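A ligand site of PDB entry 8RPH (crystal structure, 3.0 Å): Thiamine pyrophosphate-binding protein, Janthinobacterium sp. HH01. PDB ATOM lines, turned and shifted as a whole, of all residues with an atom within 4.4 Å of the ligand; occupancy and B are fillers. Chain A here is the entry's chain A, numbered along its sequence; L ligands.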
ATOM      1  N   ASP A  95     -10.763 -13.397   0.148  1.00  0.00           N
ATOM      2  CA  ASP A  95     -11.003 -13.704  -1.258  1.00  0.00           C
ATOM      3  C   ASP A  95     -12.420 -14.190  -1.546  1.00  0.00           C
ATOM      4  O   ASP A  95     -12.719 -14.536  -2.691  1.00  0.00           O
ATOM      5  CB  ASP A  95      -9.983 -14.742  -1.756  1.00  0.00           C
ATOM      6  CG  ASP A  95      -8.651 -14.127  -2.122  1.00  0.00           C
ATOM      7  OD1 ASP A  95      -8.582 -12.884  -2.243  1.00  0.00           O
ATOM      8  OD2 ASP A  95      -7.675 -14.878  -2.310  1.00  0.00           O
ATOM      9  N   SER A  96     -13.289 -14.216  -0.531  1.00  0.00           N
ATOM     10  CA  SER A  96     -14.696 -14.539  -0.742  1.00  0.00           C
ATOM     11  C   SER A  96     -14.866 -15.970  -1.231  1.00  0.00           C
ATOM     12  O   SER A  96     -15.660 -16.245  -2.131  1.00  0.00           O
ATOM     13  CB  SER A  96     -15.347 -13.553  -1.715  1.00  0.00           C
ATOM     14  OG  SER A  96     -14.912 -12.219  -1.461  1.00  0.00           O
ATOM     15  N   GLY A 161     -24.772 -15.373  -0.557  1.00  0.00           N
ATOM     16  CA  GLY A 161     -24.360 -14.025  -0.897  1.00  0.00           C
ATOM     17  C   GLY A 161     -22.903 -13.918  -1.270  1.00  0.00           C
ATOM     18  O   GLY A 161     -22.453 -14.549  -2.238  1.00  0.00           O
ATOM     19  N   ARG A 162     -22.155 -13.107  -0.531  1.00  0.00           N
ATOM     20  CA  ARG A 162     -20.714 -13.048  -0.707  1.00  0.00           C
ATOM     21  C   ARG A 162     -20.090 -14.240   0.021  1.00  0.00           C
ATOM     22  O   ARG A 162     -20.091 -14.263   1.263  1.00  0.00           O
ATOM     23  CB  ARG A 162     -20.143 -11.738  -0.179  1.00  0.00           C
ATOM     24  CG  ARG A 162     -18.663 -11.579  -0.443  1.00  0.00           C
ATOM     25  CD  ARG A 162     -18.125 -10.265   0.083  1.00  0.00           C
ATOM     26  NE  ARG A 162     -16.702 -10.132  -0.169  1.00  0.00           N
ATOM     27  CZ  ARG A 162     -15.954  -9.120   0.258  1.00  0.00           C
ATOM     28  NH1 ARG A 162     -16.473  -8.143   0.997  1.00  0.00           N
ATOM     29  NH2 ARG A 162     -14.669  -9.089  -0.069  1.00  0.00           N
ATOM     30  N   PRO A 163     -19.563 -15.233  -0.684  1.00  0.00           N
ATOM     31  CA  PRO A 163     -19.086 -16.445  -0.014  1.00  0.00           C
ATOM     32  C   PRO A 163     -17.970 -16.154   0.970  1.00  0.00           C
ATOM     33  O   PRO A 163     -17.394 -15.064   1.003  1.00  0.00           O
ATOM     34  CB  PRO A 163     -18.598 -17.328  -1.171  1.00  0.00           C
ATOM     35  CG  PRO A 163     -19.266 -16.786  -2.389  1.00  0.00           C
ATOM     36  CD  PRO A 163     -19.406 -15.320  -2.149  1.00  0.00           C
ATOM     37  N   GLY A 222     -14.619  -9.493 -12.728  1.00  0.00           N
ATOM     38  CA  GLY A 222     -13.950 -10.017 -11.556  1.00  0.00           C
ATOM     39  C   GLY A 222     -14.437 -11.404 -11.196  1.00  0.00           C
ATOM     40  O   GLY A 222     -15.352 -11.947 -11.808  1.00  0.00           O
ATOM     41  N   ASN A 223     -13.797 -11.963 -10.157  1.00  0.00           N
ATOM     42  CA  ASN A 223     -14.086 -13.320  -9.743  1.00  0.00           C
ATOM     43  C   ASN A 223     -15.483 -13.486  -9.162  1.00  0.00           C
ATOM     44  O   ASN A 223     -15.986 -14.605  -9.081  1.00  0.00           O
ATOM     45  CB  ASN A 223     -13.056 -13.793  -8.720  1.00  0.00           C
ATOM     46  CG  ASN A 223     -13.199 -15.259  -8.378  1.00  0.00           C
ATOM     47  OD1 ASN A 223     -13.474 -16.090  -9.250  1.00  0.00           O
ATOM     48  ND2 ASN A 223     -13.020 -15.599  -7.095  1.00  0.00           N
ATOM     49  N   GLY A 224     -16.124 -12.380  -8.747  1.00  0.00           N
ATOM     50  CA  GLY A 224     -17.508 -12.477  -8.312  1.00  0.00           C
ATOM     51  C   GLY A 224     -18.397 -13.118  -9.347  1.00  0.00           C
ATOM     52  O   GLY A 224     -19.376 -13.795  -9.005  1.00  0.00           O
ATOM     53  N   LEU A 227     -17.869 -16.856  -8.961  1.00  0.00           N
ATOM     54  CA  LEU A 227     -18.524 -17.294  -7.733  1.00  0.00           C
ATOM     55  C   LEU A 227     -20.035 -17.315  -7.897  1.00  0.00           C
ATOM     56  O   LEU A 227     -20.718 -18.159  -7.305  1.00  0.00           O
ATOM     57  CB  LEU A 227     -18.127 -16.392  -6.572  1.00  0.00           C
ATOM     58  CG  LEU A 227     -16.658 -16.399  -6.155  1.00  0.00           C
ATOM     59  CD1 LEU A 227     -16.397 -15.337  -5.087  1.00  0.00           C
ATOM     60  CD2 LEU A 227     -16.234 -17.780  -5.666  1.00  0.00           C
ATOM     61  N   ALA A 228     -20.584 -16.391  -8.683  1.00  0.00           N
ATOM     62  CA  ALA A 228     -22.017 -16.361  -8.956  1.00  0.00           C
ATOM     63  C   ALA A 228     -22.450 -17.387  -9.993  1.00  0.00           C
ATOM     64  O   ALA A 228     -23.652 -17.630 -10.133  1.00  0.00           O
ATOM     65  CB  ALA A 228     -22.428 -14.965  -9.420  1.00  0.00           C
ATOM     66  N   SER A 248      -9.777  -8.880 -13.836  1.00  0.00           N
ATOM     67  CA  SER A 248      -8.978  -8.798 -12.627  1.00  0.00           C
ATOM     68  C   SER A 248      -8.069 -10.016 -12.518  1.00  0.00           C
ATOM     69  O   SER A 248      -8.292 -11.055 -13.156  1.00  0.00           O
ATOM     70  CB  SER A 248      -9.859  -8.703 -11.391  1.00  0.00           C
ATOM     71  OG  SER A 248     -10.615  -9.890 -11.221  1.00  0.00           O
ATOM     72  N   TRP A 249      -7.035  -9.893 -11.685  1.00  0.00           N
ATOM     73  CA  TRP A 249      -6.115 -11.012 -11.485  1.00  0.00           C
ATOM     74  C   TRP A 249      -6.871 -12.263 -11.045  1.00  0.00           C
ATOM     75  O   TRP A 249      -6.563 -13.375 -11.500  1.00  0.00           O
ATOM     76  CB  TRP A 249      -5.049 -10.637 -10.462  1.00  0.00           C
ATOM     77  CG  TRP A 249      -3.926  -9.812 -11.039  1.00  0.00           C
ATOM     78  CD1 TRP A 249      -3.927  -9.151 -12.234  1.00  0.00           C
ATOM     79  CD2 TRP A 249      -2.645  -9.583 -10.451  1.00  0.00           C
ATOM     80  NE1 TRP A 249      -2.716  -8.517 -12.420  1.00  0.00           N
ATOM     81  CE2 TRP A 249      -1.912  -8.766 -11.340  1.00  0.00           C
ATOM     82  CE3 TRP A 249      -2.030  -9.980  -9.260  1.00  0.00           C
ATOM     83  CZ2 TRP A 249      -0.612  -8.338 -11.079  1.00  0.00           C
ATOM     84  CZ3 TRP A 249      -0.734  -9.561  -8.997  1.00  0.00           C
ATOM     85  CH2 TRP A 249      -0.039  -8.745  -9.906  1.00  0.00           C
ATOM     86  N   ALA A 250      -7.873 -12.106 -10.182  1.00  0.00           N
ATOM     87  CA  ALA A 250      -8.619 -13.266  -9.702  1.00  0.00           C
ATOM     88  C   ALA A 250      -9.522 -13.856 -10.777  1.00  0.00           C
ATOM     89  O   ALA A 250      -9.809 -15.050 -10.742  1.00  0.00           O
ATOM     90  CB  ALA A 250      -9.436 -12.885  -8.464  1.00  0.00           C
ATOM     91  N   GLY A 251      -9.973 -13.040 -11.726  1.00  0.00           N
ATOM     92  CA  GLY A 251     -10.868 -13.501 -12.758  1.00  0.00           C
ATOM     93  C   GLY A 251     -10.211 -13.630 -14.124  1.00  0.00           C
ATOM     94  O   GLY A 251     -10.857 -13.403 -15.149  1.00  0.00           O
ATOM     95  N   ALA A 266      -5.407  -4.564 -15.510  1.00  0.00           N
ATOM     96  CA  ALA A 266      -4.852  -3.278 -15.132  1.00  0.00           C
ATOM     97  C   ALA A 266      -4.672  -3.197 -13.625  1.00  0.00           C
ATOM     98  O   ALA A 266      -5.231  -3.993 -12.866  1.00  0.00           O
ATOM     99  CB  ALA A 266      -5.759  -2.130 -15.619  1.00  0.00           C
ATOM    100  N   GLY A 267      -3.885  -2.224 -13.190  1.00  0.00           N
ATOM    101  CA  GLY A 267      -3.727  -1.944 -11.775  1.00  0.00           C
ATOM    102  C   GLY A 267      -2.343  -1.394 -11.482  1.00  0.00           C
ATOM    103  O   GLY A 267      -1.671  -0.860 -12.363  1.00  0.00           O
ATOM    104  N   VAL A 268      -1.950  -1.526 -10.212  1.00  0.00           N
ATOM    105  CA  VAL A 268      -0.628  -1.086  -9.790  1.00  0.00           C
ATOM    106  C   VAL A 268       0.456  -1.935 -10.456  1.00  0.00           C
ATOM    107  O   VAL A 268       1.487  -1.409 -10.885  1.00  0.00           O
ATOM    108  CB  VAL A 268      -0.519  -1.146  -8.252  1.00  0.00           C
ATOM    109  CG1 VAL A 268       0.894  -0.827  -7.786  1.00  0.00           C
ATOM    110  CG2 VAL A 268      -1.525  -0.185  -7.624  1.00  0.00           C
ATOM    111  N   TYR A 269       0.248  -3.244 -10.535  1.00  0.00           N
ATOM    112  CA  TYR A 269       1.082  -4.134 -11.321  1.00  0.00           C
ATOM    113  C   TYR A 269       0.400  -4.543 -12.629  1.00  0.00           C
ATOM    114  O   TYR A 269       0.589  -5.654 -13.114  1.00  0.00           O
ATOM    115  CB  TYR A 269       1.444  -5.385 -10.524  1.00  0.00           C
ATOM    116  CG  TYR A 269       2.551  -5.200  -9.523  1.00  0.00           C
ATOM    117  CD1 TYR A 269       3.881  -5.398  -9.875  1.00  0.00           C
ATOM    118  CD2 TYR A 269       2.266  -4.838  -8.212  1.00  0.00           C
ATOM    119  CE1 TYR A 269       4.892  -5.241  -8.947  1.00  0.00           C
ATOM    120  CE2 TYR A 269       3.281  -4.673  -7.287  1.00  0.00           C
ATOM    121  CZ  TYR A 269       4.592  -4.878  -7.653  1.00  0.00           C
ATOM    122  OH  TYR A 269       5.590  -4.704  -6.725  1.00  0.00           O
ATOM    123  N   GLY A 270      -0.400  -3.640 -13.198  1.00  0.00           N
ATOM    124  CA  GLY A 270      -1.091  -3.943 -14.421  1.00  0.00           C
ATOM    125  C   GLY A 270      -0.183  -3.913 -15.630  1.00  0.00           C
ATOM    126  O   GLY A 270       1.006  -3.569 -15.552  1.00  0.00           O
ATOM    127  N   GLY A 288     -18.554  -7.923 -10.535  1.00  0.00           N
ATOM    128  CA  GLY A 288     -17.920  -8.979  -9.775  1.00  0.00           C
ATOM    129  C   GLY A 288     -16.507  -8.699  -9.322  1.00  0.00           C
ATOM    130  O   GLY A 288     -15.877  -9.599  -8.747  1.00  0.00           O
ATOM    131  N   THR A 289     -15.982  -7.499  -9.534  1.00  0.00           N
ATOM    132  CA  THR A 289     -14.637  -7.142  -9.121  1.00  0.00           C
ATOM    133  C   THR A 289     -14.697  -6.143  -7.977  1.00  0.00           C
ATOM    134  O   THR A 289     -15.549  -5.238  -7.967  1.00  0.00           O
ATOM    135  CB  THR A 289     -13.828  -6.562 -10.298  1.00  0.00           C
ATOM    136  OG1 THR A 289     -12.507  -6.239  -9.849  1.00  0.00           O
ATOM    137  CG2 THR A 289     -14.495  -5.311 -10.857  1.00  0.00           C
ATOM    138  N   ARG A 290     -13.791  -6.297  -7.012  1.00  0.00           N
ATOM    139  CA  ARG A 290     -13.806  -5.520  -5.777  1.00  0.00           C
ATOM    140  C   ARG A 290     -13.158  -4.156  -5.923  1.00  0.00           C
ATOM    141  O   ARG A 290     -13.260  -3.336  -5.003  1.00  0.00           O
ATOM    142  CB  ARG A 290     -13.107  -6.312  -4.659  1.00  0.00           C
ATOM    143  CG  ARG A 290     -13.106  -5.627  -3.302  1.00  0.00           C
ATOM    144  CD  ARG A 290     -12.697  -6.611  -2.195  1.00  0.00           C
ATOM    145  NE  ARG A 290     -11.388  -7.194  -2.443  1.00  0.00           N
ATOM    146  CZ  ARG A 290     -10.249  -6.732  -1.952  1.00  0.00           C
ATOM    147  NH1 ARG A 290     -10.210  -5.676  -1.158  1.00  0.00           N
ATOM    148  NH2 ARG A 290      -9.109  -7.352  -2.270  1.00  0.00           N
ATOM    149  N   ALA A 292     -10.079  -3.263  -5.688  1.00  0.00           N
ATOM    150  CA  ALA A 292      -9.183  -3.083  -4.561  1.00  0.00           C
ATOM    151  C   ALA A 292      -8.120  -2.038  -4.904  1.00  0.00           C
ATOM    152  O   ALA A 292      -8.079  -1.478  -6.002  1.00  0.00           O
ATOM    153  CB  ALA A 292      -8.541  -4.410  -4.179  1.00  0.00           C
ATOM    154  N   PRO A 294      -4.723  -2.312  -5.168  1.00  0.00           N
ATOM    155  CA  PRO A 294      -3.819  -2.683  -6.263  1.00  0.00           C
ATOM    156  C   PRO A 294      -4.450  -2.594  -7.645  1.00  0.00           C
ATOM    157  O   PRO A 294      -3.717  -2.612  -8.642  1.00  0.00           O
ATOM    158  CB  PRO A 294      -3.437  -4.135  -5.927  1.00  0.00           C
ATOM    159  CG  PRO A 294      -3.629  -4.241  -4.461  1.00  0.00           C
ATOM    160  CD  PRO A 294      -4.806  -3.370  -4.147  1.00  0.00           C
ATOM    161  N   GLN A 295      -5.780  -2.475  -7.733  1.00  0.00           N
ATOM    162  CA  GLN A 295      -6.458  -2.374  -9.019  1.00  0.00           C
ATOM    163  C   GLN A 295      -6.640  -0.937  -9.485  1.00  0.00           C
ATOM    164  O   GLN A 295      -6.427  -0.630 -10.661  1.00  0.00           O
ATOM    165  CB  GLN A 295      -7.833  -3.041  -8.948  1.00  0.00           C
ATOM    166  CG  GLN A 295      -7.802  -4.548  -8.743  1.00  0.00           C
ATOM    167  CD  GLN A 295      -9.180  -5.163  -8.789  1.00  0.00           C
ATOM    168  OE1 GLN A 295      -9.890  -5.190  -7.788  1.00  0.00           O
ATOM    169  NE2 GLN A 295      -9.567  -5.642  -9.964  1.00  0.00           N
ATOM    170  N   ASP A 313     -21.826  -5.459  -7.426  1.00  0.00           N
ATOM    171  CA  ASP A 313     -21.224  -6.246  -6.356  1.00  0.00           C
ATOM    172  C   ASP A 313     -22.337  -6.697  -5.419  1.00  0.00           C
ATOM    173  O   ASP A 313     -23.224  -5.913  -5.084  1.00  0.00           O
ATOM    174  CB  ASP A 313     -20.169  -5.425  -5.602  1.00  0.00           C
ATOM    175  CG  ASP A 313     -19.266  -6.293  -4.740  1.00  0.00           C
ATOM    176  OD1 ASP A 313     -19.791  -7.148  -3.999  1.00  0.00           O
ATOM    177  OD2 ASP A 313     -18.034  -6.103  -4.800  1.00  0.00           O
ATOM    178  N   ILE A 314     -22.275  -7.962  -4.990  1.00  0.00           N
ATOM    179  CA  ILE A 314     -23.325  -8.502  -4.147  1.00  0.00           C
ATOM    180  C   ILE A 314     -23.232  -7.964  -2.719  1.00  0.00           C
ATOM    181  O   ILE A 314     -24.210  -8.025  -1.973  1.00  0.00           O
ATOM    182  CB  ILE A 314     -23.267 -10.042  -4.155  1.00  0.00           C
ATOM    183  CG1 ILE A 314     -24.614 -10.622  -3.717  1.00  0.00           C
ATOM    184  CG2 ILE A 314     -22.148 -10.545  -3.258  1.00  0.00           C
ATOM    185  CD1 ILE A 314     -24.709 -12.112  -3.916  1.00  0.00           C
ATOM    186  N   ASP A 315     -22.065  -7.439  -2.335  1.00  0.00           N
ATOM    187  CA  ASP A 315     -21.848  -6.900  -0.996  1.00  0.00           C
ATOM    188  C   ASP A 315     -22.128  -5.402  -1.010  1.00  0.00           C
ATOM    189  O   ASP A 315     -21.458  -4.651  -1.716  1.00  0.00           O
ATOM    190  CB  ASP A 315     -20.422  -7.189  -0.545  1.00  0.00           C
ATOM    191  CG  ASP A 315     -20.205  -6.948   0.936  1.00  0.00           C
ATOM    192  OD1 ASP A 315     -20.687  -5.919   1.449  1.00  0.00           O
ATOM    193  OD2 ASP A 315     -19.558  -7.796   1.580  1.00  0.00           O
ATOM    194  N   GLU A 318     -19.005  -3.204  -0.220  1.00  0.00           N
ATOM    195  CA  GLU A 318     -18.051  -3.137  -1.333  1.00  0.00           C
ATOM    196  C   GLU A 318     -18.614  -2.318  -2.486  1.00  0.00           C
ATOM    197  O   GLU A 318     -17.850  -1.716  -3.249  1.00  0.00           O
ATOM    198  CB  GLU A 318     -17.688  -4.548  -1.800  1.00  0.00           C
ATOM    199  CG  GLU A 318     -17.027  -5.414  -0.741  1.00  0.00           C
ATOM    200  CD  GLU A 318     -15.630  -4.942  -0.390  1.00  0.00           C
ATOM    201  OE1 GLU A 318     -15.129  -4.009  -1.046  1.00  0.00           O
ATOM    202  OE2 GLU A 318     -15.025  -5.511   0.544  1.00  0.00           O
ATOM    203  N   CYS A 332     -26.149  -6.390  -6.439  1.00  0.00           N
ATOM    204  CA  CYS A 332     -26.852  -7.478  -7.107  1.00  0.00           C
ATOM    205  C   CYS A 332     -25.884  -8.602  -7.431  1.00  0.00           C
ATOM    206  O   CYS A 332     -24.693  -8.378  -7.646  1.00  0.00           O
ATOM    207  CB  CYS A 332     -27.526  -6.969  -8.391  1.00  0.00           C
ATOM    208  SG  CYS A 332     -28.572  -8.172  -9.221  1.00  0.00           S
ATOM    209  N   ASP A 333     -26.417  -9.828  -7.456  1.00  0.00           N
ATOM    210  CA  ASP A 333     -25.630 -10.986  -7.859  1.00  0.00           C
ATOM    211  C   ASP A 333     -25.123 -10.821  -9.290  1.00  0.00           C
ATOM    212  O   ASP A 333     -25.841 -10.328 -10.164  1.00  0.00           O
ATOM    213  CB  ASP A 333     -26.473 -12.256  -7.741  1.00  0.00           C
ATOM    214  CG  ASP A 333     -25.716 -13.503  -8.168  1.00  0.00           C
ATOM    215  OD1 ASP A 333     -25.659 -13.766  -9.383  1.00  0.00           O
ATOM    216  OD2 ASP A 333     -25.182 -14.209  -7.289  1.00  0.00           O
ATOM    217  N   ALA A 334     -23.888 -11.248  -9.531  1.00  0.00           N
ATOM    218  CA  ALA A 334     -23.242 -11.000 -10.808  1.00  0.00           C
ATOM    219  C   ALA A 334     -23.944 -11.732 -11.941  1.00  0.00           C
ATOM    220  O   ALA A 334     -24.049 -11.202 -13.054  1.00  0.00           O
ATOM    221  CB  ALA A 334     -21.766 -11.396 -10.742  1.00  0.00           C
ATOM    222  N   LEU A 411       3.773 -14.761  -8.475  1.00  0.00           N
ATOM    223  CA  LEU A 411       2.546 -13.972  -8.543  1.00  0.00           C
ATOM    224  C   LEU A 411       2.651 -12.853  -9.562  1.00  0.00           C
ATOM    225  O   LEU A 411       1.796 -12.717 -10.443  1.00  0.00           O
ATOM    226  CB  LEU A 411       2.228 -13.416  -7.159  1.00  0.00           C
ATOM    227  CG  LEU A 411       1.093 -12.384  -7.053  1.00  0.00           C
ATOM    228  CD1 LEU A 411      -0.268 -13.059  -7.144  1.00  0.00           C
ATOM    229  CD2 LEU A 411       1.221 -11.617  -5.751  1.00  0.00           C
ATOM    230  N   LEU A 412       3.713 -12.031  -9.461  1.00  0.00           N
ATOM    231  CA  LEU A 412       3.794 -10.827 -10.280  1.00  0.00           C
ATOM    232  C   LEU A 412       4.091 -11.166 -11.739  1.00  0.00           C
ATOM    233  O   LEU A 412       3.370 -10.754 -12.646  1.00  0.00           O
ATOM    234  CB  LEU A 412       4.857  -9.892  -9.714  1.00  0.00           C
ATOM    235  CG  LEU A 412       4.660  -9.452  -8.265  1.00  0.00           C
ATOM    236  CD1 LEU A 412       5.844  -8.601  -7.800  1.00  0.00           C
ATOM    237  CD2 LEU A 412       3.347  -8.683  -8.090  1.00  0.00           C
ATOM    238  N   THR A 430      -5.034 -13.490  -3.275  1.00  0.00           N
ATOM    239  CA  THR A 430      -4.714 -12.091  -3.504  1.00  0.00           C
ATOM    240  C   THR A 430      -5.281 -11.151  -2.455  1.00  0.00           C
ATOM    241  O   THR A 430      -4.736 -10.058  -2.265  1.00  0.00           O
ATOM    242  CB  THR A 430      -5.220 -11.666  -4.892  1.00  0.00           C
ATOM    243  OG1 THR A 430      -6.536 -12.182  -5.096  1.00  0.00           O
ATOM    244  CG2 THR A 430      -4.295 -12.171  -5.974  1.00  0.00           C
ATOM    245  N   GLY A 431      -6.359 -11.547  -1.764  1.00  0.00           N
ATOM    246  CA  GLY A 431      -6.905 -10.691  -0.724  1.00  0.00           C
ATOM    247  C   GLY A 431      -5.983 -10.546   0.468  1.00  0.00           C
ATOM    248  O   GLY A 431      -5.752  -9.447   0.961  1.00  0.00           O
ATOM    249  N   MET A 492      10.978  -9.270  -3.607  1.00  0.00           N
ATOM    250  CA  MET A 492       9.930  -8.254  -3.619  1.00  0.00           C
ATOM    251  C   MET A 492      10.156  -7.223  -2.522  1.00  0.00           C
ATOM    252  O   MET A 492       9.861  -6.038  -2.706  1.00  0.00           O
ATOM    253  CB  MET A 492       8.563  -8.925  -3.485  1.00  0.00           C
ATOM    254  CG  MET A 492       7.393  -8.001  -3.718  1.00  0.00           C
ATOM    255  SD  MET A 492       5.878  -8.888  -4.110  1.00  0.00           S
ATOM    256  CE  MET A 492       4.707  -7.538  -3.949  1.00  0.00           C
HETATM  257  P1  LIG L   1     -11.850 -10.286  -5.198  1.00  0.00           P
HETATM  258  O1  LIG L   1     -12.040 -11.561  -4.460  1.00  0.00           O
HETATM  259  O2  LIG L   1     -11.102  -9.187  -4.440  1.00  0.00           O
HETATM  260  O3  LIG L   1     -13.225  -9.723  -5.694  1.00  0.00           O
HETATM  261  C1  LIG L   1     -14.465 -10.398  -5.405  1.00  0.00           C
HETATM  262  C2  LIG L   1     -15.572  -9.375  -5.380  1.00  0.00           C
HETATM  263  O4  LIG L   1     -16.778  -9.959  -5.941  1.00  0.00           O
HETATM  264  C3  LIG L   1     -15.939  -8.893  -3.976  1.00  0.00           C
HETATM  265  O5  LIG L   1     -16.226  -7.499  -3.964  1.00  0.00           O
HETATM  266  C4  LIG L   1     -17.172  -9.741  -3.638  1.00  0.00           C
HETATM  267  O6  LIG L   1     -18.031  -9.111  -2.701  1.00  0.00           O
HETATM  268  C5  LIG L   1     -17.832  -9.834  -5.013  1.00  0.00           C
HETATM  269  N1  LIG L   1     -18.723 -10.981  -5.166  1.00  0.00           N
HETATM  270  C6  LIG L   1     -18.614 -12.198  -4.548  1.00  0.00           C
HETATM  271  N2  LIG L   1     -19.573 -13.041  -4.856  1.00  0.00           N
HETATM  272  C7  LIG L   1     -20.381 -12.315  -5.724  1.00  0.00           C
HETATM  273  C8  LIG L   1     -21.571 -12.644  -6.401  1.00  0.00           C
HETATM  274  N3  LIG L   1     -22.176 -13.827  -6.309  1.00  0.00           N
HETATM  275  N4  LIG L   1     -22.117 -11.690  -7.195  1.00  0.00           N
HETATM  276  C9  LIG L   1     -21.512 -10.507  -7.288  1.00  0.00           C
HETATM  277  N5  LIG L   1     -20.393 -10.092  -6.694  1.00  0.00           N
HETATM  278  C10 LIG L   1     -19.871 -11.041  -5.916  1.00  0.00           C
HETATM  279  N6  LIG L   1      -5.265  -7.087  -9.329  1.00  0.00           N
HETATM  280  C11 LIG L   1      -5.378  -6.459 -10.537  1.00  0.00           C
HETATM  281  O7  LIG L   1      -6.445  -6.470 -11.173  1.00  0.00           O
HETATM  282  N7  LIG L   1      -4.292  -5.783 -11.059  1.00  0.00           N
HETATM  283  C12 LIG L   1      -3.041  -5.671 -10.478  1.00  0.00           C
HETATM  284  O8  LIG L   1      -2.152  -5.046 -11.049  1.00  0.00           O
HETATM  285  C13 LIG L   1      -2.932  -6.351  -9.194  1.00  0.00           C
HETATM  286  N8  LIG L   1      -1.790  -6.301  -8.577  1.00  0.00           N
HETATM  287  C14 LIG L   1      -1.685  -6.947  -7.363  1.00  0.00           C
HETATM  288  C15 LIG L   1      -0.465  -6.900  -6.684  1.00  0.00           C
HETATM  289  C16 LIG L   1      -0.296  -7.538  -5.459  1.00  0.00           C
HETATM  290  C17 LIG L   1       1.049  -7.455  -4.770  1.00  0.00           C
HETATM  291  C18 LIG L   1      -1.372  -8.233  -4.881  1.00  0.00           C
HETATM  292  C19 LIG L   1      -1.231  -8.928  -3.561  1.00  0.00           C
HETATM  293  C20 LIG L   1      -2.593  -8.280  -5.561  1.00  0.00           C
HETATM  294  C21 LIG L   1      -2.761  -7.643  -6.786  1.00  0.00           C
HETATM  295  N9  LIG L   1      -3.979  -7.676  -7.491  1.00  0.00           N
HETATM  296  C22 LIG L   1      -4.105  -7.030  -8.699  1.00  0.00           C
HETATM  297  C23 LIG L   1      -5.156  -8.375  -6.959  1.00  0.00           C
HETATM  298  C24 LIG L   1      -6.251  -7.426  -6.483  1.00  0.00           C
HETATM  299  O9  LIG L   1      -5.690  -6.423  -5.627  1.00  0.00           O
HETATM  300  C25 LIG L   1      -7.310  -8.195  -5.702  1.00  0.00           C
HETATM  301  O10 LIG L   1      -6.685  -8.915  -4.644  1.00  0.00           O
HETATM  302  C26 LIG L   1      -8.154  -9.177  -6.524  1.00  0.00           C
HETATM  303  O11 LIG L   1      -7.326 -10.229  -7.026  1.00  0.00           O
HETATM  304  C27 LIG L   1      -8.886  -8.503  -7.658  1.00  0.00           C
HETATM  305  O12 LIG L   1      -9.729  -9.471  -8.312  1.00  0.00           O
HETATM  306  P2  LIG L   1     -11.232  -9.683  -7.870  1.00  0.00           P
HETATM  307  O13 LIG L   1     -11.849  -8.339  -7.474  1.00  0.00           O
HETATM  308  O14 LIG L   1     -11.976 -10.439  -8.900  1.00  0.00           O
HETATM  309  O15 LIG L   1     -11.071 -10.553  -6.558  1.00  0.00           O
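The indole nitrogen (NE1) of Trp 249 sits close to a nitrogen (N7) of the ligand (3.4 Å). An oxygen (O4) of the ligand lies close to the backbone carbonyl oxygen (O) of Gly 288 (3.0 Å). Residues that only touch the ligand: Pro 294 (3.2 Å), Ala 228 (3.3 Å), Gly 222 (3.3 Å), Ala 250 (3.4 Å), Asp 95 (3.5 Å), Gly 224 (3.5 Å), Pro 163 (3.5 Å), Gly 267 (3.6 Å), Val 268 (3.6 Å), Asp 315 (3.7 Å), Met 492 (3.7 Å), Ala 292 (3.8 Å), Cys 332 (3.8 Å), Leu 227 (3.9 Å), Gly 431 (3.9 Å), Glu 318 (3.9 Å) and Ser 96 (3.998 Å). 33 residues have an atom within 4 Å of the ligand: Asp 95, Ser 96, Arg 162, Pro 163, Gly 222, Asn 223, Gly 224, Leu 227, Ala 228, Ser 248, Trp 249, Ala 250, Ala 266, Gly 267, Val 268, Tyr 269, Gly 270, Gly 288, Thr 289, Arg 290, Ala 292, Pro 294, Gln 295, Asp 313, Ile 314, Asp 315, Glu 318, Cys 332, Asp 333, Ala 334, Thr 430, Gly 431 and Met 492.
The side-chain carboxylate of Asp 313 is in hydrogen-bond range of an oxygen (O5) of the ligand, 2.4 Å away. O14 of the ligand sits at hydrogen-bond distance from N of Asn 223. O of Ala 266 sits at hydrogen-bond distance from N7 of the ligand, 2.7 Å away. The side-chain hydroxyl (OG) of Ser 248 sits at hydrogen-bond distance from an oxygen (O14) of the ligand (2.7 Å). An oxygen (O13) of the ligand lies within hydrogen-bond range of the backbone NH (N) of Arg 290, at 2.9 Å. The guanidinium group (NE) of Arg 290 lies within salt-bridge range of an oxygen (O2) of the ligand. The backbone carbonyl oxygen (O) of Thr 430 lies close to an oxygen (O10) of the ligand (3.3 Å). OG1 of Thr 430 is in hydrogen-bond range of O11 of the ligand. A nitrogen (N4) of the ligand lies within hydrogen-bond range of the backbone NH (N) of Ala 334 (3.0 Å). NE of Arg 162 lies close to O6 of the ligand, 3.0 Å away. An oxygen (O8) of the ligand lies close to the backbone NH of Tyr 269 (3.0 Å). An oxygen (O8) of the ligand is in hydrogen-bond range of the backbone NH of Gly 270 (3.1 Å). The side-chain carboxylate (OD2) of Asp 333 lies within hydrogen-bond range of a nitrogen (N3) of the ligand, 3.2 Å away. O13 of the ligand is in hydrogen-bond range of OG1 of Thr 289 (3.2 Å). N of Ile 314 sits at hydrogen-bond distance from N5 of the ligand. The side-chain amide nitrogen of Gln 295 lies close to an oxygen (O7) of the ligand, at 3.4 Å.
The backbone NH of Cys 332 sits at hydrogen-bond distance from the backbone carbonyl oxygen of Asp 313 (3.3 Å). OG of Ser 248 is in hydrogen-bond range of N of Gly 251 (3.3 Å). The backbone NH of Thr 430 is in hydrogen-bond range of the side-chain carboxylate of Asp 95 (3.1 Å). O of Gly 288 sits at hydrogen-bond distance from N of Gly 224, 2.8 Å away. NH1 of Arg 162 is in salt-bridge range of OE2 of Glu 318 (3.0 Å). The guanidinium group (NE) of Arg 162 is in hydrogen-bond range of the side-chain hydroxyl (OG) of Ser 96 (3.0 Å). OG1 of Thr 289 sits at hydrogen-bond distance from NE2 of Gln 295 (3.0 Å). The side-chain amide oxygen (OE1) of Gln 295 is in hydrogen-bond range of the backbone NH (N) of Ala 292 (2.9 Å).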
